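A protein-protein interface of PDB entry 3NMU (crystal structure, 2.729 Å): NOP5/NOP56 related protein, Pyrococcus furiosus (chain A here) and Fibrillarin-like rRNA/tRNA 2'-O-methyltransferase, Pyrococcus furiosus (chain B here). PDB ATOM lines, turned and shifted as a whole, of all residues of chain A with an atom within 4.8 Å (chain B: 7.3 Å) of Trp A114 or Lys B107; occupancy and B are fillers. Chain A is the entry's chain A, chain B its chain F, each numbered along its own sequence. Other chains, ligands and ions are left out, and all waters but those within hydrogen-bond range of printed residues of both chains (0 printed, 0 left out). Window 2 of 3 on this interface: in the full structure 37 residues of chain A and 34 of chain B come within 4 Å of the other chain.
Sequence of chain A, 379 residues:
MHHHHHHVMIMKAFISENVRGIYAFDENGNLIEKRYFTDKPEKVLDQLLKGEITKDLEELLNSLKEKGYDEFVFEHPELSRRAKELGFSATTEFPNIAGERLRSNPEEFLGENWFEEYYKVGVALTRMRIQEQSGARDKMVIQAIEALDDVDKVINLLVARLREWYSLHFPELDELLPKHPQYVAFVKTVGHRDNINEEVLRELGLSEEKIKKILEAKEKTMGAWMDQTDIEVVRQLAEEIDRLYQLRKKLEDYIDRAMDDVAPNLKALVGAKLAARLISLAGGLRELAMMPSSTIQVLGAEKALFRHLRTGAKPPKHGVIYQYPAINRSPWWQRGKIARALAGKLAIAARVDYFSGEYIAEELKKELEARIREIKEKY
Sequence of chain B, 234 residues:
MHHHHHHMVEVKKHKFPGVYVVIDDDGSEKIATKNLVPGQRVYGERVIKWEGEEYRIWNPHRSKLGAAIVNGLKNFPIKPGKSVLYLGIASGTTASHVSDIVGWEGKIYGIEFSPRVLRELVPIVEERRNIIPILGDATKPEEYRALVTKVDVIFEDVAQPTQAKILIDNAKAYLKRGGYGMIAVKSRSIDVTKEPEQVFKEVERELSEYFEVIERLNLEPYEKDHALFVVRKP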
ATOM      1  N   PRO A 106      22.019  33.968  12.249  1.00  0.00           N
ATOM      2  CA  PRO A 106      22.355  35.149  11.467  1.00  0.00           C
ATOM      3  C   PRO A 106      21.111  35.804  10.877  1.00  0.00           C
ATOM      4  O   PRO A 106      21.094  37.022  10.757  1.00  0.00           O
ATOM      5  CB  PRO A 106      23.256  34.583  10.370  1.00  0.00           C
ATOM      6  CG  PRO A 106      23.823  33.319  10.943  1.00  0.00           C
ATOM      7  CD  PRO A 106      22.698  32.760  11.749  1.00  0.00           C
ATOM      8  N   GLU A 107      20.085  35.030  10.526  1.00  0.00           N
ATOM      9  CA  GLU A 107      18.888  35.628   9.924  1.00  0.00           C
ATOM     10  C   GLU A 107      18.185  36.590  10.882  1.00  0.00           C
ATOM     11  O   GLU A 107      17.563  37.573  10.444  1.00  0.00           O
ATOM     12  CB  GLU A 107      17.883  34.577   9.418  1.00  0.00           C
ATOM     13  CG  GLU A 107      16.546  35.223   9.002  1.00  0.00           C
ATOM     14  CD  GLU A 107      15.562  34.282   8.319  1.00  0.00           C
ATOM     15  OE1 GLU A 107      15.922  33.117   8.033  1.00  0.00           O
ATOM     16  OE2 GLU A 107      14.420  34.727   8.064  1.00  0.00           O
ATOM     17  N   LEU A 110      20.345  39.712  10.102  1.00  0.00           N
ATOM     18  CA  LEU A 110      20.532  40.124   8.704  1.00  0.00           C
ATOM     19  C   LEU A 110      19.414  39.833   7.693  1.00  0.00           C
ATOM     20  O   LEU A 110      19.523  40.233   6.532  1.00  0.00           O
ATOM     21  CB  LEU A 110      21.835  39.518   8.178  1.00  0.00           C
ATOM     22  CG  LEU A 110      23.176  40.151   8.565  1.00  0.00           C
ATOM     23  CD1 LEU A 110      23.182  40.690   9.988  1.00  0.00           C
ATOM     24  CD2 LEU A 110      24.284  39.129   8.382  1.00  0.00           C
ATOM     25  N   GLY A 111      18.358  39.137   8.106  1.00  0.00           N
ATOM     26  CA  GLY A 111      17.346  38.677   7.159  1.00  0.00           C
ATOM     27  C   GLY A 111      17.794  37.454   6.371  1.00  0.00           C
ATOM     28  O   GLY A 111      18.953  37.062   6.463  1.00  0.00           O
ATOM     29  N   GLU A 112      16.889  36.865   5.583  1.00  0.00           N
ATOM     30  CA  GLU A 112      17.126  35.552   4.941  1.00  0.00           C
ATOM     31  C   GLU A 112      18.192  35.529   3.828  1.00  0.00           C
ATOM     32  O   GLU A 112      18.696  34.464   3.450  1.00  0.00           O
ATOM     33  CB  GLU A 112      15.807  34.941   4.431  1.00  0.00           C
ATOM     34  CG  GLU A 112      15.489  35.205   2.952  1.00  0.00           C
ATOM     35  CD  GLU A 112      15.935  34.073   2.025  1.00  0.00           C
ATOM     36  OE1 GLU A 112      15.806  32.886   2.416  1.00  0.00           O
ATOM     37  OE2 GLU A 112      16.409  34.378   0.902  1.00  0.00           O
ATOM     38  N   ASN A 113      18.562  36.702   3.335  1.00  0.00           N
ATOM     39  CA  ASN A 113      19.609  36.795   2.332  1.00  0.00           C
ATOM     40  C   ASN A 113      20.940  36.867   3.059  1.00  0.00           C
ATOM     41  O   ASN A 113      21.975  37.151   2.466  1.00  0.00           O
ATOM     42  CB  ASN A 113      19.432  38.020   1.449  1.00  0.00           C
ATOM     43  CG  ASN A 113      17.985  38.406   1.278  1.00  0.00           C
ATOM     44  OD1 ASN A 113      17.644  39.598   1.256  1.00  0.00           O
ATOM     45  ND2 ASN A 113      17.114  37.400   1.172  1.00  0.00           N
ATOM     46  N   TRP A 114      20.897  36.639   4.365  1.00  0.00           N
ATOM     47  CA  TRP A 114      22.079  36.795   5.192  1.00  0.00           C
ATOM     48  C   TRP A 114      23.299  36.172   4.541  1.00  0.00           C
ATOM     49  O   TRP A 114      24.362  36.804   4.494  1.00  0.00           O
ATOM     50  CB  TRP A 114      21.859  36.198   6.584  1.00  0.00           C
ATOM     51  CG  TRP A 114      21.532  34.734   6.636  1.00  0.00           C
ATOM     52  CD1 TRP A 114      20.292  34.165   6.574  1.00  0.00           C
ATOM     53  CD2 TRP A 114      22.449  33.663   6.823  1.00  0.00           C
ATOM     54  NE1 TRP A 114      20.383  32.795   6.694  1.00  0.00           N
ATOM     55  CE2 TRP A 114      21.711  32.460   6.852  1.00  0.00           C
ATOM     56  CE3 TRP A 114      23.842  33.590   6.965  1.00  0.00           C
ATOM     57  CZ2 TRP A 114      22.297  31.217   7.007  1.00  0.00           C
ATOM     58  CZ3 TRP A 114      24.433  32.351   7.127  1.00  0.00           C
ATOM     59  CH2 TRP A 114      23.664  31.184   7.142  1.00  0.00           C
ATOM     60  N   PHE A 115      23.155  34.952   4.018  1.00  0.00           N
ATOM     61  CA  PHE A 115      24.310  34.309   3.413  1.00  0.00           C
ATOM     62  C   PHE A 115      24.777  35.059   2.181  1.00  0.00           C
ATOM     63  O   PHE A 115      25.983  35.168   1.931  1.00  0.00           O
ATOM     64  CB  PHE A 115      24.074  32.856   3.045  1.00  0.00           C
ATOM     65  CG  PHE A 115      25.270  32.232   2.406  1.00  0.00           C
ATOM     66  CD1 PHE A 115      25.368  32.142   1.039  1.00  0.00           C
ATOM     67  CD2 PHE A 115      26.332  31.814   3.178  1.00  0.00           C
ATOM     68  CE1 PHE A 115      26.478  31.605   0.458  1.00  0.00           C
ATOM     69  CE2 PHE A 115      27.438  31.273   2.602  1.00  0.00           C
ATOM     70  CZ  PHE A 115      27.514  31.170   1.239  1.00  0.00           C
ATOM     71  N   GLU A 116      23.819  35.559   1.403  1.00  0.00           N
ATOM     72  CA  GLU A 116      24.128  36.362   0.223  1.00  0.00           C
ATOM     73  C   GLU A 116      24.970  37.586   0.598  1.00  0.00           C
ATOM     74  O   GLU A 116      25.933  37.925  -0.096  1.00  0.00           O
ATOM     75  CB  GLU A 116      22.845  36.827  -0.466  1.00  0.00           C
ATOM     76  CG  GLU A 116      21.937  35.735  -1.007  1.00  0.00           C
ATOM     77  CD  GLU A 116      20.878  36.322  -1.929  1.00  0.00           C
ATOM     78  OE1 GLU A 116      20.292  35.577  -2.752  1.00  0.00           O
ATOM     79  OE2 GLU A 116      20.646  37.553  -1.837  1.00  0.00           O
ATOM     80  N   GLU A 117      24.596  38.254   1.689  1.00  0.00           N
ATOM     81  CA  GLU A 117      25.379  39.371   2.192  1.00  0.00           C
ATOM     82  C   GLU A 117      26.741  38.860   2.638  1.00  0.00           C
ATOM     83  O   GLU A 117      27.768  39.359   2.183  1.00  0.00           O
ATOM     84  CB  GLU A 117      24.663  40.084   3.340  1.00  0.00           C
ATOM     85  CG  GLU A 117      25.260  41.441   3.678  1.00  0.00           C
ATOM     86  CD  GLU A 117      24.474  42.157   4.752  1.00  0.00           C
ATOM     87  OE1 GLU A 117      23.408  41.627   5.143  1.00  0.00           O
ATOM     88  OE2 GLU A 117      24.921  43.244   5.200  1.00  0.00           O
ATOM     89  N   TYR A 118      26.756  37.840   3.491  1.00  0.00           N
ATOM     90  CA  TYR A 118      28.018  37.260   3.935  1.00  0.00           C
ATOM     91  C   TYR A 118      28.891  36.968   2.710  1.00  0.00           C
ATOM     92  O   TYR A 118      30.123  36.893   2.801  1.00  0.00           O
ATOM     93  CB  TYR A 118      27.766  35.980   4.725  1.00  0.00           C
ATOM     94  CG  TYR A 118      27.704  36.158   6.224  1.00  0.00           C
ATOM     95  CD1 TYR A 118      28.858  36.076   6.998  1.00  0.00           C
ATOM     96  CD2 TYR A 118      26.497  36.383   6.868  1.00  0.00           C
ATOM     97  CE1 TYR A 118      28.819  36.237   8.356  1.00  0.00           C
ATOM     98  CE2 TYR A 118      26.445  36.547   8.232  1.00  0.00           C
ATOM     99  CZ  TYR A 118      27.610  36.474   8.974  1.00  0.00           C
ATOM    100  OH  TYR A 118      27.566  36.628  10.347  1.00  0.00           O
ATOM    101  N   GLY B  81      22.095  21.166   0.767  1.00  0.00           N
ATOM    102  CA  GLY B  81      21.497  22.027   1.766  1.00  0.00           C
ATOM    103  C   GLY B  81      22.436  22.314   2.915  1.00  0.00           C
ATOM    104  O   GLY B  81      22.280  23.313   3.629  1.00  0.00           O
ATOM    105  N   LYS B  82      23.428  21.448   3.082  1.00  0.00           N
ATOM    106  CA  LYS B  82      24.311  21.517   4.235  1.00  0.00           C
ATOM    107  C   LYS B  82      25.242  22.719   4.151  1.00  0.00           C
ATOM    108  O   LYS B  82      25.604  23.142   3.059  1.00  0.00           O
ATOM    109  CB  LYS B  82      25.130  20.234   4.351  1.00  0.00           C
ATOM    110  CG  LYS B  82      24.340  19.019   4.800  1.00  0.00           C
ATOM    111  CD  LYS B  82      23.561  19.305   6.069  1.00  0.00           C
ATOM    112  CE  LYS B  82      23.130  18.032   6.782  1.00  0.00           C
ATOM    113  NZ  LYS B  82      22.363  18.367   8.025  1.00  0.00           N
ATOM    114  N   SER B  83      25.633  23.288   5.286  1.00  0.00           N
ATOM    115  CA  SER B  83      26.658  24.322   5.235  1.00  0.00           C
ATOM    116  C   SER B  83      27.972  23.713   5.704  1.00  0.00           C
ATOM    117  O   SER B  83      27.966  22.889   6.607  1.00  0.00           O
ATOM    118  CB  SER B  83      26.255  25.583   6.027  1.00  0.00           C
ATOM    119  OG  SER B  83      26.230  25.397   7.439  1.00  0.00           O
ATOM    120  N   VAL B  84      29.085  24.085   5.066  1.00  0.00           N
ATOM    121  CA  VAL B  84      30.399  23.514   5.400  1.00  0.00           C
ATOM    122  C   VAL B  84      31.545  24.523   5.397  1.00  0.00           C
ATOM    123  O   VAL B  84      31.675  25.323   4.475  1.00  0.00           O
ATOM    124  CB  VAL B  84      30.759  22.294   4.493  1.00  0.00           C
ATOM    125  CG1 VAL B  84      29.784  22.162   3.348  1.00  0.00           C
ATOM    126  CG2 VAL B  84      32.191  22.376   3.977  1.00  0.00           C
ATOM    127  N   LEU B  85      32.368  24.478   6.439  1.00  0.00           N
ATOM    128  CA  LEU B  85      33.566  25.295   6.539  1.00  0.00           C
ATOM    129  C   LEU B  85      34.751  24.510   5.966  1.00  0.00           C
ATOM    130  O   LEU B  85      35.160  23.509   6.536  1.00  0.00           O
ATOM    131  CB  LEU B  85      33.819  25.656   8.011  1.00  0.00           C
ATOM    132  CG  LEU B  85      35.182  26.284   8.390  1.00  0.00           C
ATOM    133  CD1 LEU B  85      35.506  27.553   7.565  1.00  0.00           C
ATOM    134  CD2 LEU B  85      35.308  26.570   9.889  1.00  0.00           C
ATOM    135  N   VAL B  98      32.206  19.470  -3.819  1.00  0.00           N
ATOM    136  CA  VAL B  98      31.304  19.600  -2.678  1.00  0.00           C
ATOM    137  C   VAL B  98      30.385  20.808  -2.810  1.00  0.00           C
ATOM    138  O   VAL B  98      29.414  20.946  -2.066  1.00  0.00           O
ATOM    139  CB  VAL B  98      32.039  19.638  -1.341  1.00  0.00           C
ATOM    140  CG1 VAL B  98      33.523  19.607  -1.562  1.00  0.00           C
ATOM    141  CG2 VAL B  98      31.632  20.831  -0.575  1.00  0.00           C
ATOM    142  N   VAL B 102      26.386  20.151  -2.182  1.00  0.00           N
ATOM    143  CA  VAL B 102      25.705  21.135  -1.367  1.00  0.00           C
ATOM    144  C   VAL B 102      24.562  21.835  -2.117  1.00  0.00           C
ATOM    145  O   VAL B 102      23.446  21.928  -1.621  1.00  0.00           O
ATOM    146  CB  VAL B 102      26.738  22.158  -0.877  1.00  0.00           C
ATOM    147  CG1 VAL B 102      26.096  23.476  -0.588  1.00  0.00           C
ATOM    148  CG2 VAL B 102      27.473  21.602   0.328  1.00  0.00           C
ATOM    149  N   GLY B 103      24.832  22.330  -3.318  1.00  0.00           N
ATOM    150  CA  GLY B 103      23.770  22.918  -4.120  1.00  0.00           C
ATOM    151  C   GLY B 103      23.488  24.379  -3.840  1.00  0.00           C
ATOM    152  O   GLY B 103      24.252  25.034  -3.145  1.00  0.00           O
ATOM    153  N   TRP B 104      22.391  24.901  -4.378  1.00  0.00           N
ATOM    154  CA  TRP B 104      22.105  26.324  -4.235  1.00  0.00           C
ATOM    155  C   TRP B 104      21.687  26.650  -2.826  1.00  0.00           C
ATOM    156  O   TRP B 104      21.994  27.729  -2.309  1.00  0.00           O
ATOM    157  CB  TRP B 104      21.024  26.798  -5.208  1.00  0.00           C
ATOM    158  CG  TRP B 104      21.504  26.896  -6.612  1.00  0.00           C
ATOM    159  CD1 TRP B 104      20.932  26.329  -7.714  1.00  0.00           C
ATOM    160  CD2 TRP B 104      22.660  27.572  -7.073  1.00  0.00           C
ATOM    161  NE1 TRP B 104      21.658  26.624  -8.838  1.00  0.00           N
ATOM    162  CE2 TRP B 104      22.753  27.403  -8.464  1.00  0.00           C
ATOM    163  CE3 TRP B 104      23.662  28.331  -6.448  1.00  0.00           C
ATOM    164  CZ2 TRP B 104      23.754  27.930  -9.244  1.00  0.00           C
ATOM    165  CZ3 TRP B 104      24.666  28.863  -7.208  1.00  0.00           C
ATOM    166  CH2 TRP B 104      24.709  28.664  -8.590  1.00  0.00           C
ATOM    167  N   GLU B 105      21.005  25.707  -2.200  1.00  0.00           N
ATOM    168  CA  GLU B 105      20.444  25.948  -0.896  1.00  0.00           C
ATOM    169  C   GLU B 105      21.493  25.734   0.181  1.00  0.00           C
ATOM    170  O   GLU B 105      21.218  25.867   1.381  1.00  0.00           O
ATOM    171  CB  GLU B 105      19.202  25.087  -0.706  1.00  0.00           C
ATOM    172  CG  GLU B 105      18.058  25.626  -1.533  1.00  0.00           C
ATOM    173  CD  GLU B 105      17.924  27.130  -1.337  1.00  0.00           C
ATOM    174  OE1 GLU B 105      18.072  27.908  -2.316  1.00  0.00           O
ATOM    175  OE2 GLU B 105      17.695  27.540  -0.175  1.00  0.00           O
ATOM    176  N   GLY B 106      22.706  25.428  -0.262  1.00  0.00           N
ATOM    177  CA  GLY B 106      23.822  25.228   0.639  1.00  0.00           C
ATOM    178  C   GLY B 106      24.789  26.389   0.694  1.00  0.00           C
ATOM    179  O   GLY B 106      24.641  27.360  -0.050  1.00  0.00           O
ATOM    180  N   LYS B 107      25.782  26.280   1.576  1.00  0.00           N
ATOM    181  CA  LYS B 107      26.727  27.360   1.868  1.00  0.00           C
ATOM    182  C   LYS B 107      28.111  26.774   2.091  1.00  0.00           C
ATOM    183  O   LYS B 107      28.262  25.833   2.856  1.00  0.00           O
ATOM    184  CB  LYS B 107      26.300  28.101   3.146  1.00  0.00           C
ATOM    185  CG  LYS B 107      24.982  28.871   3.046  1.00  0.00           C
ATOM    186  CD  LYS B 107      24.018  28.519   4.181  1.00  0.00           C
ATOM    187  CE  LYS B 107      22.822  29.481   4.259  1.00  0.00           C
ATOM    188  NZ  LYS B 107      21.715  29.147   3.310  1.00  0.00           N
ATOM    189  N   ILE B 108      29.128  27.319   1.447  1.00  0.00           N
ATOM    190  CA  ILE B 108      30.494  26.920   1.776  1.00  0.00           C
ATOM    191  C   ILE B 108      31.377  28.117   2.143  1.00  0.00           C
ATOM    192  O   ILE B 108      31.282  29.164   1.507  1.00  0.00           O
ATOM    193  CB  ILE B 108      31.147  26.219   0.615  1.00  0.00           C
ATOM    194  CG1 ILE B 108      30.208  25.139   0.087  1.00  0.00           C
ATOM    195  CG2 ILE B 108      32.464  25.668   1.069  1.00  0.00           C
ATOM    196  CD1 ILE B 108      30.775  24.259  -1.031  1.00  0.00           C
ATOM    197  N   TYR B 109      32.231  27.978   3.153  1.00  0.00           N
ATOM    198  CA  TYR B 109      33.171  29.042   3.492  1.00  0.00           C
ATOM    199  C   TYR B 109      34.565  28.514   3.203  1.00  0.00           C
ATOM    200  O   TYR B 109      35.084  27.694   3.954  1.00  0.00           O
ATOM    201  CB  TYR B 109      33.059  29.405   4.992  1.00  0.00           C
ATOM    202  CG  TYR B 109      31.702  29.929   5.381  1.00  0.00           C
ATOM    203  CD1 TYR B 109      30.896  29.242   6.250  1.00  0.00           C
ATOM    204  CD2 TYR B 109      31.212  31.100   4.838  1.00  0.00           C
ATOM    205  CE1 TYR B 109      29.636  29.709   6.584  1.00  0.00           C
ATOM    206  CE2 TYR B 109      29.951  31.578   5.160  1.00  0.00           C
ATOM    207  CZ  TYR B 109      29.162  30.875   6.037  1.00  0.00           C
ATOM    208  OH  TYR B 109      27.900  31.341   6.375  1.00  0.00           O
ATOM    209  N   ARG B 129      27.553  30.734  -6.459  1.00  0.00           N
ATOM    210  CA  ARG B 129      27.317  31.810  -5.517  1.00  0.00           C
ATOM    211  C   ARG B 129      27.306  31.258  -4.095  1.00  0.00           C
ATOM    212  O   ARG B 129      27.097  31.994  -3.111  1.00  0.00           O
ATOM    213  CB  ARG B 129      26.048  32.596  -5.884  1.00  0.00           C
ATOM    214  CG  ARG B 129      26.222  33.527  -7.102  1.00  0.00           C
ATOM    215  CD  ARG B 129      25.714  34.956  -6.823  1.00  0.00           C
ATOM    216  NE  ARG B 129      26.794  35.946  -6.664  1.00  0.00           N
ATOM    217  CZ  ARG B 129      27.375  36.599  -7.674  1.00  0.00           C
ATOM    218  NH1 ARG B 129      26.998  36.380  -8.938  1.00  0.00           N
ATOM    219  NH2 ARG B 129      28.343  37.471  -7.429  1.00  0.00           N
ATOM    220  N   ASN B 130      27.556  29.949  -4.017  1.00  0.00           N
ATOM    221  CA  ASN B 130      27.564  29.189  -2.767  1.00  0.00           C
ATOM    222  C   ASN B 130      28.944  28.930  -2.169  1.00  0.00           C
ATOM    223  O   ASN B 130      29.053  28.209  -1.178  1.00  0.00           O
ATOM    224  CB  ASN B 130      26.789  27.877  -2.918  1.00  0.00           C
ATOM    225  CG  ASN B 130      27.497  26.883  -3.814  1.00  0.00           C
ATOM    226  OD1 ASN B 130      28.644  27.069  -4.189  1.00  0.00           O
ATOM    227  ND2 ASN B 130      26.818  25.807  -4.139  1.00  0.00           N
ATOM    228  N   ILE B 131      29.997  29.465  -2.779  1.00  0.00           N
ATOM    229  CA  ILE B 131      31.289  29.512  -2.102  1.00  0.00           C
ATOM    230  C   ILE B 131      31.737  30.937  -1.832  1.00  0.00           C
ATOM    231  O   ILE B 131      31.701  31.787  -2.724  1.00  0.00           O
ATOM    232  CB  ILE B 131      32.394  28.864  -2.892  1.00  0.00           C
ATOM    233  CG1 ILE B 131      32.026  27.441  -3.259  1.00  0.00           C
ATOM    234  CG2 ILE B 131      33.673  28.870  -2.092  1.00  0.00           C
ATOM    235  CD1 ILE B 131      33.011  26.847  -4.213  1.00  0.00           C
ATOM    236  N   ILE B 132      32.160  31.194  -0.595  1.00  0.00           N
ATOM    237  CA  ILE B 132      32.797  32.455  -0.273  1.00  0.00           C
ATOM    238  C   ILE B 132      34.283  32.173  -0.177  1.00  0.00           C
ATOM    239  O   ILE B 132      34.703  31.398   0.664  1.00  0.00           O
ATOM    240  CB  ILE B 132      32.285  33.022   1.043  1.00  0.00           C
ATOM    241  CG1 ILE B 132      30.764  33.136   1.014  1.00  0.00           C
ATOM    242  CG2 ILE B 132      32.885  34.374   1.293  1.00  0.00           C
ATOM    243  CD1 ILE B 132      30.154  33.516   2.329  1.00  0.00           C
ATOM    244  N   VAL B 148      32.363  34.194   8.650  1.00  0.00           N
ATOM    245  CA  VAL B 148      31.686  32.901   8.613  1.00  0.00           C
ATOM    246  C   VAL B 148      30.502  32.807   9.584  1.00  0.00           C
ATOM    247  O   VAL B 148      30.178  33.770  10.245  1.00  0.00           O
ATOM    248  CB  VAL B 148      32.679  31.756   8.913  1.00  0.00           C
ATOM    249  CG1 VAL B 148      34.007  32.001   8.205  1.00  0.00           C
ATOM    250  CG2 VAL B 148      32.904  31.647  10.379  1.00  0.00           C
ATOM    251  N   THR B 149      29.839  31.654   9.632  1.00  0.00           N
ATOM    252  CA  THR B 149      28.736  31.396  10.568  1.00  0.00           C
ATOM    253  C   THR B 149      28.694  29.899  10.859  1.00  0.00           C
ATOM    254  O   THR B 149      29.222  29.129  10.078  1.00  0.00           O
ATOM    255  CB  THR B 149      27.349  31.851  10.034  1.00  0.00           C
ATOM    256  OG1 THR B 149      26.897  30.958   9.010  1.00  0.00           O
ATOM    257  CG2 THR B 149      27.406  33.275   9.501  1.00  0.00           C
ATOM    258  N   LYS B 150      28.069  29.476  11.956  1.00  0.00           N
ATOM    259  CA  LYS B 150      28.138  28.073  12.364  1.00  0.00           C
ATOM    260  C   LYS B 150      27.775  27.171  11.186  1.00  0.00           C
ATOM    261  O   LYS B 150      26.823  27.448  10.453  1.00  0.00           O
ATOM    262  CB  LYS B 150      27.240  27.800  13.589  1.00  0.00           C
ATOM    263  CG  LYS B 150      27.705  28.470  14.915  1.00  0.00           C
ATOM    264  CD  LYS B 150      28.073  27.462  16.020  1.00  0.00           C
ATOM    265  CE  LYS B 150      26.880  27.121  16.946  1.00  0.00           C
ATOM    266  NZ  LYS B 150      25.600  26.599  16.307  1.00  0.00           N
ATOM    267  N   VAL B 151      28.542  26.095  11.004  1.00  0.00           N
ATOM    268  CA  VAL B 151      28.347  25.203   9.873  1.00  0.00           C
ATOM    269  C   VAL B 151      27.850  23.804  10.306  1.00  0.00           C
ATOM    270  O   VAL B 151      27.835  23.472  11.498  1.00  0.00           O
ATOM    271  CB  VAL B 151      29.687  25.036   9.115  1.00  0.00           C
ATOM    272  CG1 VAL B 151      30.091  26.335   8.399  1.00  0.00           C
ATOM    273  CG2 VAL B 151      30.782  24.590  10.066  1.00  0.00           C
ATOM    274  N   ASP B 152      27.453  22.986   9.332  1.00  0.00           N
ATOM    275  CA  ASP B 152      27.047  21.602   9.581  1.00  0.00           C
ATOM    276  C   ASP B 152      28.239  20.665   9.590  1.00  0.00           C
ATOM    277  O   ASP B 152      28.237  19.647  10.268  1.00  0.00           O
ATOM    278  CB  ASP B 152      26.019  21.126   8.552  1.00  0.00           C
ATOM    279  CG  ASP B 152      24.654  21.797   8.717  1.00  0.00           C
ATOM    280  OD1 ASP B 152      24.310  22.707   7.924  1.00  0.00           O
ATOM    281  OD2 ASP B 152      23.905  21.391   9.628  1.00  0.00           O
ATOM    282  N   VAL B 153      29.251  21.011   8.812  1.00  0.00           N
ATOM    283  CA  VAL B 153      30.384  20.135   8.588  1.00  0.00           C
ATOM    284  C   VAL B 153      31.657  20.951   8.442  1.00  0.00           C
ATOM    285  O   VAL B 153      31.614  22.077   7.974  1.00  0.00           O
ATOM    286  CB  VAL B 153      30.203  19.354   7.273  1.00  0.00           C
ATOM    287  CG1 VAL B 153      31.410  18.462   7.006  1.00  0.00           C
ATOM    288  CG2 VAL B 153      28.890  18.556   7.273  1.00  0.00           C
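Of the 11 printed residues of chain A, 4 touch a printed residue of chain B.
Hydrophobic or aromatic side chains of chain A that line the printed part of chain B: Pro A106, Trp A114, Phe A115 and Tyr A118.
Hydrophobic or aromatic side chains of chain B within 4 Å of the printed part of chain A: Tyr B109 and Ile B132.
Thr B149 touches Pro A106.
CE of Lys B107 touches CZ2 of Trp A114, at 3.3 Å.
Trp A114 touches Tyr B109.
Trp A114 touches Thr B149 (CZ3 to OG1, 3.4 Å).
Phe A115 touches Lys B107 (CD2 to CG, 3.2 Å).
Phe A115 touches Tyr B109.
Phe A115 touches Arg B129.
Phe A115 touches Ile B132 (CE2 to CD1, 3.5 Å).
Tyr A118 touches Val B148.
Tyr A118 touches Thr B149.
O of Lys B82 sits at hydrogen-bond distance from N of Lys B107.
The backbone NH of Val B84 sits at hydrogen-bond distance from the backbone carbonyl oxygen of Lys B107, 2.9 Å away.
OG1 of Thr B149 lies within hydrogen-bond range of OH of Tyr B109 (2.8 Å).
O of Ile B108 lies within hydrogen-bond range of N of Ile B132, at 3.1 Å.
N of Tyr B109 is in hydrogen-bond range of O of Val B84 (3.0 Å).
Of the printed residues of chain B, Pro A106 touches Thr B149.
Of chain B, only Lys B107 (3.3 Å), Tyr B109 (3.7 Å) and Thr B149 (3.4 Å) come within 4 Å of Trp A114.
Gly B106 touches none of the printed residues of chain A.
Of chain A, only Trp A114 (3.3 Å) and Phe A115 (3.2 Å) come within 4 Å of Lys B107.
Printed residues of chain A within 4 Å of Arg B129: Phe A115 (3.6 Å).
Ile B131 touches none of the printed residues of chain A.
Of the printed residues of chain A, Ile B132 touches Phe A115 and Tyr A118.
Of the printed residues of chain A, Val B148 touches Tyr A118.
Printed residues of chain A within 4 Å of Thr B149: Pro A106, Trp A114 and Tyr A118.
The nearest residue of chain B that does not touch Trp A114 is Lys B150 (5.9 Å).
The nearest printed residue of chain A that does not touch Lys B107 is Glu A112 (6.1 Å).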
